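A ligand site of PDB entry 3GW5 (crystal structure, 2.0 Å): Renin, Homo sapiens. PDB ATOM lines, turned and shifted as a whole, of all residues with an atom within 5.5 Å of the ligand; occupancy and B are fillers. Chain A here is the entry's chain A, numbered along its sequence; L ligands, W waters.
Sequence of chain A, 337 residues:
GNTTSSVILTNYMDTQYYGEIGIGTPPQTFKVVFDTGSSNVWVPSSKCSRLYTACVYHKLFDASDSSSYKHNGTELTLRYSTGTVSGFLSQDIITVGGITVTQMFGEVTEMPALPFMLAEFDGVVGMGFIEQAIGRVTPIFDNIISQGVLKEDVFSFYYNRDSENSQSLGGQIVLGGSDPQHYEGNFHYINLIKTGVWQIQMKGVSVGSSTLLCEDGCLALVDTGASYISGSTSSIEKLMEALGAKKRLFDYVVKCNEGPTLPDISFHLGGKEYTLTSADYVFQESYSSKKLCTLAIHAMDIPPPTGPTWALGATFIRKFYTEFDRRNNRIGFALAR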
ATOM      1  N   THR A  15      12.165  27.601 -16.009  1.00  0.00           N
ATOM      2  CA  THR A  15      12.740  26.276 -16.186  1.00  0.00           C
ATOM      3  C   THR A  15      14.197  26.304 -16.634  1.00  0.00           C
ATOM      4  O   THR A  15      14.951  25.396 -16.308  1.00  0.00           O
ATOM      5  CB  THR A  15      11.922  25.416 -17.205  1.00  0.00           C
ATOM      6  OG1 THR A  15      12.138  25.908 -18.528  1.00  0.00           O
ATOM      7  CG2 THR A  15      10.430  25.491 -16.891  1.00  0.00           C
ATOM      8  N   GLN A  16      14.609  27.342 -17.366  1.00  0.00           N
ATOM      9  CA  GLN A  16      16.017  27.472 -17.739  1.00  0.00           C
ATOM     10  C   GLN A  16      16.633  28.765 -17.225  1.00  0.00           C
ATOM     11  O   GLN A  16      16.162  29.852 -17.542  1.00  0.00           O
ATOM     12  CB  GLN A  16      16.179  27.398 -19.261  1.00  0.00           C
ATOM     13  CG  GLN A  16      15.708  26.091 -19.879  1.00  0.00           C
ATOM     14  CD  GLN A  16      15.987  26.014 -21.370  1.00  0.00           C
ATOM     15  OE1 GLN A  16      16.994  26.547 -21.840  1.00  0.00           O
ATOM     16  NE2 GLN A  16      15.115  25.349 -22.114  1.00  0.00           N
ATOM     17  N   TYR A  17      17.697  28.641 -16.434  1.00  0.00           N
ATOM     18  CA  TYR A  17      18.421  29.813 -15.951  1.00  0.00           C
ATOM     19  C   TYR A  17      19.846  29.794 -16.481  1.00  0.00           C
ATOM     20  O   TYR A  17      20.558  28.810 -16.321  1.00  0.00           O
ATOM     21  CB  TYR A  17      18.466  29.836 -14.418  1.00  0.00           C
ATOM     22  CG  TYR A  17      17.132  30.037 -13.758  1.00  0.00           C
ATOM     23  CD1 TYR A  17      16.800  31.268 -13.199  1.00  0.00           C
ATOM     24  CD2 TYR A  17      16.204  29.018 -13.697  1.00  0.00           C
ATOM     25  CE1 TYR A  17      15.572  31.471 -12.596  1.00  0.00           C
ATOM     26  CE2 TYR A  17      14.972  29.209 -13.087  1.00  0.00           C
ATOM     27  CZ  TYR A  17      14.674  30.439 -12.541  1.00  0.00           C
ATOM     28  OH  TYR A  17      13.468  30.622 -11.915  1.00  0.00           O
ATOM     29  N   VAL A  33      24.843  27.753 -18.894  1.00  0.00           N
ATOM     30  CA  VAL A  33      24.316  27.352 -17.599  1.00  0.00           C
ATOM     31  C   VAL A  33      25.467  27.212 -16.599  1.00  0.00           C
ATOM     32  O   VAL A  33      26.499  26.602 -16.903  1.00  0.00           O
ATOM     33  CB  VAL A  33      23.606  25.983 -17.701  1.00  0.00           C
ATOM     34  CG1 VAL A  33      23.040  25.603 -16.348  1.00  0.00           C
ATOM     35  CG2 VAL A  33      22.502  26.053 -18.738  1.00  0.00           C
ATOM     36  N   ASP A  35      26.474  25.352 -13.501  1.00  0.00           N
ATOM     37  CA  ASP A  35      25.929  24.081 -13.081  1.00  0.00           C
ATOM     38  C   ASP A  35      26.765  23.480 -11.952  1.00  0.00           C
ATOM     39  O   ASP A  35      27.883  23.017 -12.189  1.00  0.00           O
ATOM     40  CB  ASP A  35      25.895  23.134 -14.284  1.00  0.00           C
ATOM     41  CG  ASP A  35      25.427  21.729 -13.907  1.00  0.00           C
ATOM     42  OD1 ASP A  35      24.569  21.593 -13.008  1.00  0.00           O
ATOM     43  OD2 ASP A  35      25.915  20.753 -14.524  1.00  0.00           O
ATOM     44  N   GLY A  37      26.193  20.809 -10.496  1.00  0.00           N
ATOM     45  CA  GLY A  37      26.192  19.370 -10.618  1.00  0.00           C
ATOM     46  C   GLY A  37      27.240  18.823 -11.560  1.00  0.00           C
ATOM     47  O   GLY A  37      27.381  17.602 -11.711  1.00  0.00           O
ATOM     48  N   SER A  38      27.981  19.704 -12.221  1.00  0.00           N
ATOM     49  CA  SER A  38      29.063  19.258 -13.089  1.00  0.00           C
ATOM     50  C   SER A  38      30.224  20.230 -13.015  1.00  0.00           C
ATOM     51  O   SER A  38      30.120  21.283 -12.374  1.00  0.00           O
ATOM     52  CB  SER A  38      28.570  19.115 -14.534  1.00  0.00           C
ATOM     53  OG  SER A  38      28.222  20.354 -15.091  1.00  0.00           O
ATOM     54  N   TRP A  42      32.276  24.125 -21.321  1.00  0.00           N
ATOM     55  CA  TRP A  42      32.251  23.876 -22.763  1.00  0.00           C
ATOM     56  C   TRP A  42      31.296  24.787 -23.502  1.00  0.00           C
ATOM     57  O   TRP A  42      30.294  25.251 -22.937  1.00  0.00           O
ATOM     58  CB  TRP A  42      31.913  22.400 -23.045  1.00  0.00           C
ATOM     59  CG  TRP A  42      30.512  21.978 -22.674  1.00  0.00           C
ATOM     60  CD1 TRP A  42      30.112  21.386 -21.507  1.00  0.00           C
ATOM     61  CD2 TRP A  42      29.344  22.064 -23.501  1.00  0.00           C
ATOM     62  NE1 TRP A  42      28.768  21.102 -21.566  1.00  0.00           N
ATOM     63  CE2 TRP A  42      28.274  21.501 -22.769  1.00  0.00           C
ATOM     64  CE3 TRP A  42      29.096  22.565 -24.786  1.00  0.00           C
ATOM     65  CZ2 TRP A  42      26.975  21.408 -23.291  1.00  0.00           C
ATOM     66  CZ3 TRP A  42      27.808  22.480 -25.303  1.00  0.00           C
ATOM     67  CH2 TRP A  42      26.764  21.909 -24.555  1.00  0.00           C
ATOM     68  N   TYR A  80      26.097  13.540 -19.772  1.00  0.00           N
ATOM     69  CA  TYR A  80      25.126  13.885 -18.739  1.00  0.00           C
ATOM     70  C   TYR A  80      23.961  12.902 -18.849  1.00  0.00           C
ATOM     71  O   TYR A  80      23.845  12.194 -19.849  1.00  0.00           O
ATOM     72  CB  TYR A  80      24.619  15.317 -18.922  1.00  0.00           C
ATOM     73  CG  TYR A  80      25.722  16.367 -18.992  1.00  0.00           C
ATOM     74  CD1 TYR A  80      26.222  16.964 -17.843  1.00  0.00           C
ATOM     75  CD2 TYR A  80      26.244  16.762 -20.226  1.00  0.00           C
ATOM     76  CE1 TYR A  80      27.205  17.936 -17.911  1.00  0.00           C
ATOM     77  CE2 TYR A  80      27.220  17.738 -20.305  1.00  0.00           C
ATOM     78  CZ  TYR A  80      27.706  18.325 -19.151  1.00  0.00           C
ATOM     79  OH  TYR A  80      28.648  19.319 -19.245  1.00  0.00           O
ATOM     80  N   SER A  81      23.115  12.849 -17.833  1.00  0.00           N
ATOM     81  CA  SER A  81      21.959  11.949 -17.869  1.00  0.00           C
ATOM     82  C   SER A  81      21.167  12.185 -19.135  1.00  0.00           C
ATOM     83  O   SER A  81      20.709  11.240 -19.782  1.00  0.00           O
ATOM     84  CB  SER A  81      21.063  12.193 -16.649  1.00  0.00           C
ATOM     85  OG  SER A  81      21.632  11.692 -15.450  1.00  0.00           O
ATOM     86  N   THR A  82      21.024  13.461 -19.502  1.00  0.00           N
ATOM     87  CA  THR A  82      20.120  13.897 -20.560  1.00  0.00           C
ATOM     88  C   THR A  82      20.746  13.893 -21.954  1.00  0.00           C
ATOM     89  O   THR A  82      20.110  14.301 -22.928  1.00  0.00           O
ATOM     90  CB  THR A  82      19.598  15.307 -20.265  1.00  0.00           C
ATOM     91  OG1 THR A  82      18.763  15.767 -21.331  1.00  0.00           O
ATOM     92  CG2 THR A  82      20.765  16.254 -20.099  1.00  0.00           C
ATOM     93  N   GLY A  83      21.994  13.440 -22.060  1.00  0.00           N
ATOM     94  CA  GLY A  83      22.619  13.370 -23.363  1.00  0.00           C
ATOM     95  C   GLY A  83      24.099  13.711 -23.351  1.00  0.00           C
ATOM     96  O   GLY A  83      24.597  14.359 -22.434  1.00  0.00           O
ATOM     97  N   PRO A 115      19.167  16.793 -25.999  1.00  0.00           N
ATOM     98  CA  PRO A 115      18.175  17.807 -25.664  1.00  0.00           C
ATOM     99  C   PRO A 115      18.439  19.213 -26.255  1.00  0.00           C
ATOM    100  O   PRO A 115      17.625  20.118 -26.068  1.00  0.00           O
ATOM    101  CB  PRO A 115      18.216  17.836 -24.153  1.00  0.00           C
ATOM    102  CG  PRO A 115      19.670  17.613 -23.854  1.00  0.00           C
ATOM    103  CD  PRO A 115      20.228  16.753 -24.977  1.00  0.00           C
ATOM    104  N   PHE A 116      19.570  19.398 -26.932  1.00  0.00           N
ATOM    105  CA  PHE A 116      20.082  20.750 -27.130  1.00  0.00           C
ATOM    106  C   PHE A 116      19.319  21.651 -28.086  1.00  0.00           C
ATOM    107  O   PHE A 116      19.437  22.871 -28.027  1.00  0.00           O
ATOM    108  CB  PHE A 116      21.572  20.694 -27.515  1.00  0.00           C
ATOM    109  CG  PHE A 116      22.440  20.195 -26.395  1.00  0.00           C
ATOM    110  CD1 PHE A 116      22.786  21.025 -25.339  1.00  0.00           C
ATOM    111  CD2 PHE A 116      22.851  18.865 -26.352  1.00  0.00           C
ATOM    112  CE1 PHE A 116      23.518  20.542 -24.252  1.00  0.00           C
ATOM    113  CE2 PHE A 116      23.583  18.366 -25.279  1.00  0.00           C
ATOM    114  CZ  PHE A 116      23.911  19.209 -24.224  1.00  0.00           C
ATOM    115  N   LEU A 118      16.479  22.147 -27.616  1.00  0.00           N
ATOM    116  CA  LEU A 118      15.570  22.785 -26.657  1.00  0.00           C
ATOM    117  C   LEU A 118      16.296  23.784 -25.758  1.00  0.00           C
ATOM    118  O   LEU A 118      15.664  24.454 -24.943  1.00  0.00           O
ATOM    119  CB  LEU A 118      14.875  21.736 -25.780  1.00  0.00           C
ATOM    120  CG  LEU A 118      14.035  20.636 -26.436  1.00  0.00           C
ATOM    121  CD1 LEU A 118      13.460  19.746 -25.352  1.00  0.00           C
ATOM    122  CD2 LEU A 118      12.927  21.229 -27.278  1.00  0.00           C
ATOM    123  N   ALA A 119      17.619  23.868 -25.879  1.00  0.00           N
ATOM    124  CA  ALA A 119      18.407  24.729 -25.006  1.00  0.00           C
ATOM    125  C   ALA A 119      18.335  26.190 -25.438  1.00  0.00           C
ATOM    126  O   ALA A 119      18.549  26.516 -26.610  1.00  0.00           O
ATOM    127  CB  ALA A 119      19.864  24.274 -24.972  1.00  0.00           C
ATOM    128  N   PHE A 121      20.375  28.234 -24.153  1.00  0.00           N
ATOM    129  CA  PHE A 121      21.752  28.638 -23.856  1.00  0.00           C
ATOM    130  C   PHE A 121      22.667  27.872 -24.811  1.00  0.00           C
ATOM    131  O   PHE A 121      22.234  26.928 -25.472  1.00  0.00           O
ATOM    132  CB  PHE A 121      22.105  28.266 -22.409  1.00  0.00           C
ATOM    133  CG  PHE A 121      21.733  26.853 -22.050  1.00  0.00           C
ATOM    134  CD1 PHE A 121      20.463  26.557 -21.551  1.00  0.00           C
ATOM    135  CD2 PHE A 121      22.619  25.809 -22.260  1.00  0.00           C
ATOM    136  CE1 PHE A 121      20.101  25.250 -21.282  1.00  0.00           C
ATOM    137  CE2 PHE A 121      22.266  24.500 -21.989  1.00  0.00           C
ATOM    138  CZ  PHE A 121      21.003  24.218 -21.507  1.00  0.00           C
ATOM    139  N   VAL A 124      27.839  25.216 -21.026  1.00  0.00           N
ATOM    140  CA  VAL A 124      27.742  25.201 -19.593  1.00  0.00           C
ATOM    141  C   VAL A 124      29.058  25.517 -18.898  1.00  0.00           C
ATOM    142  O   VAL A 124      30.144  25.199 -19.386  1.00  0.00           O
ATOM    143  CB  VAL A 124      27.195  23.845 -19.044  1.00  0.00           C
ATOM    144  CG1 VAL A 124      26.774  22.947 -20.200  1.00  0.00           C
ATOM    145  CG2 VAL A 124      28.225  23.167 -18.157  1.00  0.00           C
ATOM    146  N   TYR A 159      17.791  32.692  -7.893  1.00  0.00           N
ATOM    147  CA  TYR A 159      16.915  32.433  -9.021  1.00  0.00           C
ATOM    148  C   TYR A 159      15.610  33.124  -8.685  1.00  0.00           C
ATOM    149  O   TYR A 159      15.102  32.981  -7.580  1.00  0.00           O
ATOM    150  CB  TYR A 159      16.672  30.925  -9.191  1.00  0.00           C
ATOM    151  CG  TYR A 159      17.770  30.152  -9.897  1.00  0.00           C
ATOM    152  CD1 TYR A 159      18.869  30.790 -10.457  1.00  0.00           C
ATOM    153  CD2 TYR A 159      17.687  28.758 -10.030  1.00  0.00           C
ATOM    154  CE1 TYR A 159      19.837  30.078 -11.130  1.00  0.00           C
ATOM    155  CE2 TYR A 159      18.662  28.042 -10.692  1.00  0.00           C
ATOM    156  CZ  TYR A 159      19.735  28.705 -11.253  1.00  0.00           C
ATOM    157  OH  TYR A 159      20.696  27.979 -11.910  1.00  0.00           O
ATOM    158  N   ASP A 223      21.630  21.315  -6.894  1.00  0.00           N
ATOM    159  CA  ASP A 223      22.033  21.341  -8.287  1.00  0.00           C
ATOM    160  C   ASP A 223      21.433  22.494  -9.057  1.00  0.00           C
ATOM    161  O   ASP A 223      20.253  22.488  -9.379  1.00  0.00           O
ATOM    162  CB  ASP A 223      21.657  20.028  -8.965  1.00  0.00           C
ATOM    163  CG  ASP A 223      22.368  19.846 -10.283  1.00  0.00           C
ATOM    164  OD1 ASP A 223      22.781  20.872 -10.891  1.00  0.00           O
ATOM    165  OD2 ASP A 223      22.518  18.696 -10.701  1.00  0.00           O
ATOM    166  N   THR A 224      22.270  23.473  -9.352  1.00  0.00           N
ATOM    167  CA  THR A 224      21.789  24.689  -9.991  1.00  0.00           C
ATOM    168  C   THR A 224      21.495  24.465 -11.466  1.00  0.00           C
ATOM    169  O   THR A 224      20.747  25.240 -12.076  1.00  0.00           O
ATOM    170  CB  THR A 224      22.793  25.849  -9.797  1.00  0.00           C
ATOM    171  OG1 THR A 224      24.058  25.489 -10.375  1.00  0.00           O
ATOM    172  CG2 THR A 224      22.973  26.146  -8.304  1.00  0.00           C
ATOM    173  N   GLY A 225      22.052  23.406 -12.042  1.00  0.00           N
ATOM    174  CA  GLY A 225      21.750  23.086 -13.424  1.00  0.00           C
ATOM    175  C   GLY A 225      20.450  22.304 -13.597  1.00  0.00           C
ATOM    176  O   GLY A 225      19.990  22.102 -14.719  1.00  0.00           O
ATOM    177  N   ALA A 226      19.872  21.856 -12.487  1.00  0.00           N
ATOM    178  CA  ALA A 226      18.597  21.149 -12.519  1.00  0.00           C
ATOM    179  C   ALA A 226      17.429  22.136 -12.502  1.00  0.00           C
ATOM    180  O   ALA A 226      17.442  23.104 -11.755  1.00  0.00           O
ATOM    181  CB  ALA A 226      18.488  20.225 -11.310  1.00  0.00           C
ATOM    182  N   SER A 227      16.426  21.877 -13.334  1.00  0.00           N
ATOM    183  CA  SER A 227      15.256  22.753 -13.407  1.00  0.00           C
ATOM    184  C   SER A 227      14.202  22.408 -12.365  1.00  0.00           C
ATOM    185  O   SER A 227      13.647  23.290 -11.713  1.00  0.00           O
ATOM    186  CB  SER A 227      14.626  22.658 -14.802  1.00  0.00           C
ATOM    187  OG  SER A 227      15.571  23.035 -15.791  1.00  0.00           O
ATOM    188  N   HIS A 298      10.170  15.792 -10.656  1.00  0.00           N
ATOM    189  CA  HIS A 298      10.149  14.586 -11.482  1.00  0.00           C
ATOM    190  C   HIS A 298      11.125  13.526 -10.973  1.00  0.00           C
ATOM    191  O   HIS A 298      11.821  13.720  -9.982  1.00  0.00           O
ATOM    192  CB  HIS A 298      10.459  14.914 -12.945  1.00  0.00           C
ATOM    193  CG  HIS A 298      11.871  15.374 -13.188  1.00  0.00           C
ATOM    194  ND1 HIS A 298      12.473  15.268 -14.422  1.00  0.00           N
ATOM    195  CD2 HIS A 298      12.787  15.928 -12.363  1.00  0.00           C
ATOM    196  CE1 HIS A 298      13.713  15.729 -14.349  1.00  0.00           C
ATOM    197  NE2 HIS A 298      13.926  16.131 -13.109  1.00  0.00           N
ATOM    198  N   MET A 300      14.459  11.139 -11.413  1.00  0.00           N
ATOM    199  CA  MET A 300      15.753  11.004 -12.068  1.00  0.00           C
ATOM    200  C   MET A 300      16.610  10.030 -11.274  1.00  0.00           C
ATOM    201  O   MET A 300      16.989  10.311 -10.135  1.00  0.00           O
ATOM    202  CB  MET A 300      16.455  12.367 -12.130  1.00  0.00           C
ATOM    203  CG  MET A 300      17.711  12.352 -12.979  1.00  0.00           C
ATOM    204  SD  MET A 300      17.492  13.253 -14.523  1.00  0.00           S
ATOM    205  CE  MET A 300      18.093  14.861 -14.046  1.00  0.00           C
ATOM    206  N   ALA A 314      16.016  24.220  -9.434  1.00  0.00           N
ATOM    207  CA  ALA A 314      15.558  25.609  -9.402  1.00  0.00           C
ATOM    208  C   ALA A 314      14.244  25.760  -8.642  1.00  0.00           C
ATOM    209  O   ALA A 314      13.981  26.795  -8.047  1.00  0.00           O
ATOM    210  CB  ALA A 314      15.396  26.144 -10.814  1.00  0.00           C
HETATM  211  C1  LIG L   1      17.433  21.656 -18.482  1.00  0.00           C
HETATM  212  O1  LIG L   1      16.124  22.014 -17.991  1.00  0.00           O
HETATM  213  C2  LIG L   1      17.439  21.733 -20.063  1.00  0.00           C
HETATM  214  C3  LIG L   1      16.338  22.106 -20.944  1.00  0.00           C
HETATM  215  C4  LIG L   1      18.807  21.344 -20.663  1.00  0.00           C
HETATM  216  C5  LIG L   1      16.551  22.109 -22.392  1.00  0.00           C
HETATM  217  C6  LIG L   1      18.968  21.362 -22.100  1.00  0.00           C
HETATM  218  C7  LIG L   1      17.844  21.743 -22.963  1.00  0.00           C
HETATM  219  C8  LIG L   1      18.456  22.708 -17.896  1.00  0.00           C
HETATM  220  C9  LIG L   1      18.326  24.221 -18.257  1.00  0.00           C
HETATM  221  C10 LIG L   1      19.387  25.169 -17.653  1.00  0.00           C
HETATM  222  C11 LIG L   1      19.423  25.211 -16.108  1.00  0.00           C
HETATM  223  O2  LIG L   1      18.157  25.538 -15.602  1.00  0.00           O
HETATM  224  C12 LIG L   1      18.116  25.565 -14.197  1.00  0.00           C
HETATM  225  C13 LIG L   1      21.853  19.061 -15.252  1.00  0.00           C
HETATM  226  C14 LIG L   1      22.003  19.116 -13.695  1.00  0.00           C
HETATM  227  C15 LIG L   1      22.580  20.215 -15.991  1.00  0.00           C
HETATM  228  N1  LIG L   1      23.406  19.060 -13.255  1.00  0.00           N
HETATM  229  C16 LIG L   1      22.514  20.221 -17.543  1.00  0.00           C
HETATM  230  C17 LIG L   1      23.273  21.445 -18.130  1.00  0.00           C
HETATM  231  C18 LIG L   1      23.239  21.492 -19.697  1.00  0.00           C
HETATM  232  C19 LIG L   1      23.698  20.175 -20.390  1.00  0.00           C
HETATM  233  C20 LIG L   1      23.150  18.872 -18.166  1.00  0.00           C
HETATM  234  C21 LIG L   1      23.111  18.829 -19.744  1.00  0.00           C
HETATM  235  N2  LIG L   1      20.447  19.138 -15.614  1.00  0.00           N
HETATM  236  C22 LIG L   1      19.538  18.109 -15.795  1.00  0.00           C
HETATM  237  O3  LIG L   1      19.854  16.933 -15.656  1.00  0.00           O
HETATM  238  N3  LIG L   1      18.249  18.541 -16.140  1.00  0.00           N
HETATM  239  C23 LIG L   1      17.141  17.574 -17.980  1.00  0.00           C
HETATM  240  C24 LIG L   1      16.811  19.016 -18.484  1.00  0.00           C
HETATM  241  C25 LIG L   1      17.825  20.187 -17.947  1.00  0.00           C
HETATM  242  C26 LIG L   1      17.822  20.005 -16.326  1.00  0.00           C
HETATM  243  C27 LIG L   1      17.160  17.628 -16.394  1.00  0.00           C
HETATM  244  C28 LIG L   1      24.084  17.780 -13.532  1.00  0.00           C
HETATM  245 CL1  LIG L   1      20.449  20.936 -22.773  1.00  0.00          CL
HETATM  246  O   HOH W   1      26.052  15.435 -14.692  1.00  0.00           O
HETATM  247  O   HOH W   2      15.119  19.508 -14.163  1.00  0.00           O
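The backbone carbonyl oxygen (O) of Thr 15 lies close to an oxygen (O2) of the ligand.
Gln 16 touches the ligand (NE2 to C5, 3.6 Å).
Val 33 touches the ligand (CG2 to C10, 3.4 Å).
Gly 37 touches the ligand (O to C28, 3.8 Å).
Tyr 80 touches the ligand.
CG2 of Thr 82 touches C21 of the ligand (3.5 Å).
O of Pro 115 touches C7 of the ligand, 3.5 Å away.
CE1 of Phe 116 touches CL1 of the ligand, at 3.4 Å.
O of Leu 118 touches C5 of the ligand, at 3.6 Å.
Ala 119 touches the ligand.
CZ of Phe 121 touches C6 of the ligand (3.6 Å).
Val 124 touches the ligand (CG1 to C18, 3.9 Å).
Thr 224 touches the ligand.
O of Ala 226 touches C12 of the ligand, 3.5 Å away.
CE of Met 300 touches O3 of the ligand (3.2 Å).
20 residues have an atom within 4 Å of the ligand: Thr 15, Gln 16, Tyr 17, Val 33, Asp 35, Gly 37, Tyr 80, Thr 82, Pro 115, Phe 116, Leu 118, Ala 119, Phe 121, Val 124, Asp 223, Thr 224, Gly 225, Ala 226, Ser 227 and Met 300.
The nearest printed residue that does not touch the ligand is Tyr 159 (4.2 Å).
N of Ala 314 sits at hydrogen-bond distance from O of Ser 227 (3.4 Å).
The backbone NH (N) of Gly 37 lies within hydrogen-bond range of the side-chain carboxylate (OD1) of Asp 223, at 3.4 Å.
The side-chain carboxylate (OD1) of Asp 35 sits close to the backbone NH (N) of Gly 225, at 3.2 Å.
OD1 of Asp 35 lies within hydrogen-bond range of N of Gly 37 (3.1 Å).
The side-chain carboxylate of Asp 35 is in hydrogen-bond range of the side-chain hydroxyl of Ser 38, at 2.4 Å.
The backbone carbonyl oxygen (O) of Ala 226 lies within hydrogen-bond range of the backbone NH (N) of Ala 314 (2.9 Å).
The backbone carbonyl oxygen of Leu 118 is in hydrogen-bond range of the side-chain amide nitrogen of Gln 16, 3.0 Å away.
O of Val 124 is in hydrogen-bond range of N of Trp 42 (3.1 Å).
An oxygen (O1) of the ligand lies within hydrogen-bond range of the side-chain hydroxyl (OG) of Ser 227, at 2.5 Å.
The side-chain carboxylate (OD2) of Asp 223 lies within salt-bridge range of a nitrogen (N1) of the ligand, 2.7 Å away.
The side-chain carboxylate (OD1) of Asp 35 lies within salt-bridge range of a nitrogen (N1) of the ligand (2.8 Å).
N2 of the ligand sits at hydrogen-bond distance from O of Gly 225 (3.1 Å).
O2 of the ligand lies within hydrogen-bond range of N of Tyr 17 (3.2 Å).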
